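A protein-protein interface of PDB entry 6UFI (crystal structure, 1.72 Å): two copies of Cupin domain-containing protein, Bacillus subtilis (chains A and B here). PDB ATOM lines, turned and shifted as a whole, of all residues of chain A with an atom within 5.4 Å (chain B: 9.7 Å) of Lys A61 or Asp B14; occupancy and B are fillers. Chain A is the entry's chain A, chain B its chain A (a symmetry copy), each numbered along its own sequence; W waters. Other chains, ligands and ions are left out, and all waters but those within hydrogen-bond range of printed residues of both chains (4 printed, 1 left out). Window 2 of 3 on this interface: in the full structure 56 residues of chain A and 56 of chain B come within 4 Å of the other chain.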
ATOM      1  N   LEU A  59      -6.687  25.726  -2.007  1.00  0.00           N
ATOM      2  CA  LEU A  59      -5.334  25.598  -1.465  1.00  0.00           C
ATOM      3  C   LEU A  59      -4.593  24.468  -2.177  1.00  0.00           C
ATOM      4  O   LEU A  59      -5.133  23.369  -2.338  1.00  0.00           O
ATOM      5  CB  LEU A  59      -5.374  25.319   0.041  1.00  0.00           C
ATOM      6  CG  LEU A  59      -6.245  26.240   0.908  1.00  0.00           C
ATOM      7  CD1 LEU A  59      -6.027  25.968   2.394  1.00  0.00           C
ATOM      8  CD2 LEU A  59      -5.995  27.714   0.586  1.00  0.00           C
ATOM      9  N   GLU A  60      -3.346  24.725  -2.570  1.00  0.00           N
ATOM     10  CA  GLU A  60      -2.531  23.701  -3.217  1.00  0.00           C
ATOM     11  C   GLU A  60      -1.133  23.730  -2.620  1.00  0.00           C
ATOM     12  O   GLU A  60      -0.753  24.673  -1.923  1.00  0.00           O
ATOM     13  CB  GLU A  60      -2.445  23.910  -4.738  1.00  0.00           C
ATOM     14  CG  GLU A  60      -3.787  23.864  -5.489  1.00  0.00           C
ATOM     15  CD  GLU A  60      -4.411  22.478  -5.516  1.00  0.00           C
ATOM     16  OE1 GLU A  60      -3.730  21.484  -5.161  1.00  0.00           O
ATOM     17  OE2 GLU A  60      -5.598  22.377  -5.897  1.00  0.00           O
ATOM     18  N   LYS A  61      -0.356  22.687  -2.901  1.00  0.00           N
ATOM     19  CA  LYS A  61       1.062  22.739  -2.538  1.00  0.00           C
ATOM     20  C   LYS A  61       1.734  23.758  -3.443  1.00  0.00           C
ATOM     21  O   LYS A  61       1.892  23.521  -4.645  1.00  0.00           O
ATOM     22  CB  LYS A  61       1.716  21.369  -2.675  1.00  0.00           C
ATOM     23  CG  LYS A  61       1.085  20.295  -1.799  1.00  0.00           C
ATOM     24  CD  LYS A  61       1.882  18.999  -1.909  1.00  0.00           C
ATOM     25  CE  LYS A  61       1.295  17.913  -1.026  1.00  0.00           C
ATOM     26  NZ  LYS A  61       2.207  16.726  -0.978  1.00  0.00           N
ATOM     27  N   GLY A  62       2.090  24.908  -2.882  1.00  0.00           N
ATOM     28  CA  GLY A  62       2.650  26.000  -3.653  1.00  0.00           C
ATOM     29  C   GLY A  62       1.850  27.286  -3.629  1.00  0.00           C
ATOM     30  O   GLY A  62       2.368  28.315  -4.090  1.00  0.00           O
ATOM     31  N   GLY A  63       0.619  27.302  -3.119  1.00  0.00           N
ATOM     32  CA  GLY A  63      -0.092  28.583  -3.107  1.00  0.00           C
ATOM     33  C   GLY A  63      -1.605  28.404  -3.002  1.00  0.00           C
ATOM     34  O   GLY A  63      -2.087  27.400  -2.477  1.00  0.00           O
ATOM     35  N   LYS A  87       4.037  30.531  -3.685  1.00  0.00           N
ATOM     36  CA  LYS A  87       5.230  30.481  -2.839  1.00  0.00           C
ATOM     37  C   LYS A  87       6.489  30.573  -3.700  1.00  0.00           C
ATOM     38  O   LYS A  87       6.434  30.382  -4.915  1.00  0.00           O
ATOM     39  CB  LYS A  87       5.224  29.187  -2.035  1.00  0.00           C
ATOM     40  CG  LYS A  87       4.057  29.145  -1.044  1.00  0.00           C
ATOM     41  CD  LYS A  87       3.901  27.775  -0.406  1.00  0.00           C
ATOM     42  CE  LYS A  87       5.111  27.406   0.425  1.00  0.00           C
ATOM     43  NZ  LYS A  87       4.944  26.035   0.991  1.00  0.00           N
ATOM     44  N   ILE A 201      -1.208  24.142  -9.528  1.00  0.00           N
ATOM     45  CA  ILE A 201      -0.139  24.880  -8.859  1.00  0.00           C
ATOM     46  C   ILE A 201       0.747  23.832  -8.205  1.00  0.00           C
ATOM     47  O   ILE A 201       0.227  22.910  -7.563  1.00  0.00           O
ATOM     48  CB  ILE A 201      -0.675  25.866  -7.797  1.00  0.00           C
ATOM     49  CG1 ILE A 201      -1.356  27.072  -8.441  1.00  0.00           C
ATOM     50  CG2 ILE A 201       0.446  26.329  -6.832  1.00  0.00           C
ATOM     51  CD1 ILE A 201      -2.047  27.993  -7.421  1.00  0.00           C
ATOM     52  N   PHE A 202       2.066  23.934  -8.399  1.00  0.00           N
ATOM     53  CA  PHE A 202       2.950  22.944  -7.776  1.00  0.00           C
ATOM     54  C   PHE A 202       4.279  23.572  -7.356  1.00  0.00           C
ATOM     55  O   PHE A 202       4.727  24.562  -7.935  1.00  0.00           O
ATOM     56  CB  PHE A 202       3.186  21.717  -8.689  1.00  0.00           C
ATOM     57  CG  PHE A 202       3.758  22.026 -10.063  1.00  0.00           C
ATOM     58  CD1 PHE A 202       2.944  22.508 -11.086  1.00  0.00           C
ATOM     59  CD2 PHE A 202       5.085  21.743 -10.354  1.00  0.00           C
ATOM     60  CE1 PHE A 202       3.460  22.753 -12.367  1.00  0.00           C
ATOM     61  CE2 PHE A 202       5.613  21.972 -11.630  1.00  0.00           C
ATOM     62  CZ  PHE A 202       4.790  22.484 -12.644  1.00  0.00           C
ATOM     63  N   GLU A 203       4.892  22.989  -6.320  1.00  0.00           N
ATOM     64  CA  GLU A 203       6.164  23.495  -5.807  1.00  0.00           C
ATOM     65  C   GLU A 203       7.301  23.160  -6.771  1.00  0.00           C
ATOM     66  O   GLU A 203       7.291  22.125  -7.454  1.00  0.00           O
ATOM     67  CB  GLU A 203       6.476  22.902  -4.419  1.00  0.00           C
ATOM     68  CG  GLU A 203       5.369  23.078  -3.364  1.00  0.00           C
ATOM     69  CD  GLU A 203       5.529  24.312  -2.473  1.00  0.00           C
ATOM     70  OE1 GLU A 203       6.082  25.335  -2.919  1.00  0.00           O
ATOM     71  OE2 GLU A 203       5.071  24.262  -1.309  1.00  0.00           O
ATOM     72  N   PRO B  10      -4.612  31.057   5.163  1.00  0.00           N
ATOM     73  CA  PRO B  10      -5.108  29.985   4.274  1.00  0.00           C
ATOM     74  C   PRO B  10      -4.056  28.903   4.071  1.00  0.00           C
ATOM     75  O   PRO B  10      -3.461  28.744   2.999  1.00  0.00           O
ATOM     76  CB  PRO B  10      -5.443  30.750   2.989  1.00  0.00           C
ATOM     77  CG  PRO B  10      -4.516  31.941   3.007  1.00  0.00           C
ATOM     78  CD  PRO B  10      -4.337  32.316   4.448  1.00  0.00           C
ATOM     79  N   ILE B  11      -3.816  28.147   5.141  1.00  0.00           N
ATOM     80  CA  ILE B  11      -2.846  27.057   5.164  1.00  0.00           C
ATOM     81  C   ILE B  11      -3.523  25.819   5.735  1.00  0.00           C
ATOM     82  O   ILE B  11      -4.192  25.894   6.772  1.00  0.00           O
ATOM     83  CB  ILE B  11      -1.598  27.426   5.994  1.00  0.00           C
ATOM     84  CG1 ILE B  11      -0.829  28.548   5.296  1.00  0.00           C
ATOM     85  CG2 ILE B  11      -0.694  26.182   6.215  1.00  0.00           C
ATOM     86  CD1 ILE B  11       0.226  29.197   6.166  1.00  0.00           C
ATOM     87  N   ARG B  12      -3.381  24.694   5.038  1.00  0.00           N
ATOM     88  CA  ARG B  12      -3.871  23.395   5.498  1.00  0.00           C
ATOM     89  C   ARG B  12      -2.722  22.417   5.274  1.00  0.00           C
ATOM     90  O   ARG B  12      -2.454  22.014   4.139  1.00  0.00           O
ATOM     91  CB  ARG B  12      -5.132  22.955   4.755  1.00  0.00           C
ATOM     92  CG  ARG B  12      -5.824  21.738   5.380  1.00  0.00           C
ATOM     93  CD  ARG B  12      -6.737  21.008   4.396  1.00  0.00           C
ATOM     94  NE  ARG B  12      -7.608  21.919   3.657  1.00  0.00           N
ATOM     95  CZ  ARG B  12      -7.568  22.092   2.340  1.00  0.00           C
ATOM     96  NH1 ARG B  12      -8.398  22.953   1.748  1.00  0.00           N
ATOM     97  NH2 ARG B  12      -6.702  21.396   1.610  1.00  0.00           N
ATOM     98  N   GLY B  13      -2.032  22.072   6.345  1.00  0.00           N
ATOM     99  CA  GLY B  13      -0.894  21.168   6.212  1.00  0.00           C
ATOM    100  C   GLY B  13       0.176  21.778   5.328  1.00  0.00           C
ATOM    101  O   GLY B  13       0.673  22.886   5.590  1.00  0.00           O
ATOM    102  N   ASP B  14       0.538  21.066   4.253  1.00  0.00           N
ATOM    103  CA  ASP B  14       1.532  21.553   3.300  1.00  0.00           C
ATOM    104  C   ASP B  14       0.911  22.287   2.118  1.00  0.00           C
ATOM    105  O   ASP B  14       1.611  22.557   1.138  1.00  0.00           O
ATOM    106  CB  ASP B  14       2.413  20.397   2.796  1.00  0.00           C
ATOM    107  CG  ASP B  14       1.613  19.221   2.262  1.00  0.00           C
ATOM    108  OD1 ASP B  14       0.409  19.382   1.976  1.00  0.00           O
ATOM    109  OD2 ASP B  14       2.202  18.124   2.115  1.00  0.00           O
ATOM    110  N   LYS B  15      -0.372  22.636   2.199  1.00  0.00           N
ATOM    111  CA  LYS B  15      -1.062  23.354   1.136  1.00  0.00           C
ATOM    112  C   LYS B  15      -1.379  24.769   1.592  1.00  0.00           C
ATOM    113  O   LYS B  15      -1.545  25.030   2.790  1.00  0.00           O
ATOM    114  CB  LYS B  15      -2.360  22.646   0.735  1.00  0.00           C
ATOM    115  CG  LYS B  15      -2.132  21.242   0.159  1.00  0.00           C
ATOM    116  CD  LYS B  15      -3.436  20.610  -0.310  1.00  0.00           C
ATOM    117  CE  LYS B  15      -3.149  19.314  -1.071  1.00  0.00           C
ATOM    118  NZ  LYS B  15      -4.369  18.473  -1.261  1.00  0.00           N
ATOM    119  N   GLY B  16      -1.454  25.679   0.629  1.00  0.00           N
ATOM    120  CA  GLY B  16      -1.758  27.066   0.930  1.00  0.00           C
ATOM    121  C   GLY B  16      -0.512  27.854   1.303  1.00  0.00           C
ATOM    122  O   GLY B  16       0.624  27.384   1.171  1.00  0.00           O
ATOM    123  N   ALA B  17      -0.737  29.080   1.786  1.00  0.00           N
ATOM    124  CA  ALA B  17       0.355  30.005   2.104  1.00  0.00           C
ATOM    125  C   ALA B  17      -0.207  31.181   2.894  1.00  0.00           C
ATOM    126  O   ALA B  17      -1.421  31.359   2.991  1.00  0.00           O
ATOM    127  CB  ALA B  17       1.051  30.514   0.834  1.00  0.00           C
ATOM    128  N   VAL B  36      -9.992  28.360   4.777  1.00  0.00           N
ATOM    129  CA  VAL B  36      -9.396  27.020   4.799  1.00  0.00           C
ATOM    130  C   VAL B  36     -10.514  25.995   4.633  1.00  0.00           C
ATOM    131  O   VAL B  36     -11.047  25.469   5.624  1.00  0.00           O
ATOM    132  CB  VAL B  36      -8.579  26.764   6.082  1.00  0.00           C
ATOM    133  CG1 VAL B  36      -7.915  25.360   6.018  1.00  0.00           C
ATOM    134  CG2 VAL B  36      -7.520  27.842   6.272  1.00  0.00           C
ATOM    135  N   GLU B  39     -10.684  19.569   2.768  1.00  0.00           N
ATOM    136  CA  GLU B  39      -9.994  19.029   1.603  1.00  0.00           C
ATOM    137  C   GLU B  39     -10.942  18.283   0.673  1.00  0.00           C
ATOM    138  O   GLU B  39     -10.591  18.057  -0.490  1.00  0.00           O
ATOM    139  CB  GLU B  39      -8.845  18.112   2.024  1.00  0.00           C
ATOM    140  CG  GLU B  39      -9.263  16.827   2.692  1.00  0.00           C
ATOM    141  CD  GLU B  39      -8.065  15.968   3.059  1.00  0.00           C
ATOM    142  OE1 GLU B  39      -6.923  16.384   2.761  1.00  0.00           O
ATOM    143  OE2 GLU B  39      -8.262  14.885   3.648  1.00  0.00           O
HETATM  144  O   HOH W   1       4.953  17.595   0.198  1.00  0.00           O
HETATM  145  O   HOH W   2      -9.047  24.486  -0.603  1.00  0.00           O
HETATM  146  O   HOH W   3       4.183  22.221   0.052  1.00  0.00           O
HETATM  147  O   HOH W   4      -7.221  21.793  -1.738  1.00  0.00           O
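Printed residues of chain B that touch a printed residue of chain A: Pro B10, Arg B12, Asp B14, Lys B15, Gly B16 and Ala B17.
Hydrophobic or aromatic side chains of chain B within 4 Å of the printed part of chain A: Pro B10 and Ala B17.
Among the printed residues, 11 pairs touch across the chains.
No position is printed for both chains.
Of the 11 pairs that touch across the chains among the printed residues, none has its exchanged pair printed and touching as well.
Among the printed residues, pairs that only touch across the chains: Leu A59 with Pro B10 (3.6 Å), Leu A59 with Arg B12 (3.9 Å), Leu A59 with Lys B15 (3.8 Å), Leu A59 with Gly B16 (3.98 Å), Glu A60 with Lys B15 (3.3 Å), Lys A61 with Lys B15 (3.8 Å), Gly A63 with Gly B16 (3.4 Å), Lys A87 with Gly B16 (3.7 Å) and Lys A87 with Ala B17 (3.8 Å).
O of Pro B10 sits at hydrogen-bond distance from N of Ala B17, at 3.0 Å.
The backbone carbonyl oxygen of Gly A62 sits at hydrogen-bond distance from the backbone NH of Lys A87, 2.8 Å away.
O of Lys A61 sits at hydrogen-bond distance from N of Glu A203 (3.5 Å).
OE2 of Glu A203 is in salt-bridge range of NZ of Lys A87 (2.9 Å).
Water W3 bridges the side-chain carboxylate (OE2) of Glu A203 and the backbone carbonyl oxygen (O) of Asp B14.
Water W4 bridges the backbone carbonyl oxygen of Leu A59 and the guanidinium group of Arg B12.
Water W2 bridges NH1 of Arg B12 (2.9 Å) and N of Leu A59 (3.0 Å).
Water W1 bridges the side-chain amino group (NZ) of Lys A61 and the side-chain carboxylate (OD2) of Asp B14.
Asp B14 touches one residue of chain A.
No residue of chain B comes within 4 Å of Gly A62.
Of the printed residues of chain B, Leu A59 touches Pro B10 (3.6 Å), Arg B12 (3.9 Å), Lys B15 (3.8 Å) and Gly B16 (3.98 Å).
Printed residues of chain A within 4 Å of Ala B17: Lys A87 (3.8 Å).
Printed residues of chain A within 4 Å of Gly B16: Leu A59 (3.98 Å), Glu A60 (2.8 Å), Gly A63 (3.4 Å) and Lys A87 (3.7 Å).
Of the printed residues of chain B, Glu A60 touches Lys B15 (3.3 Å) and Gly B16 (2.8 Å).
The nearest printed residue of chain A that does not touch Arg B12 is Glu A60 (6.3 Å).
The backbone NH (N) of Gly B16 is in hydrogen-bond range of the backbone carbonyl oxygen (O) of Glu A60 (2.8 Å).
The side-chain carboxylate of Asp B14 is in salt-bridge range of the side-chain amino group of Lys A61, 3.4 Å away.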
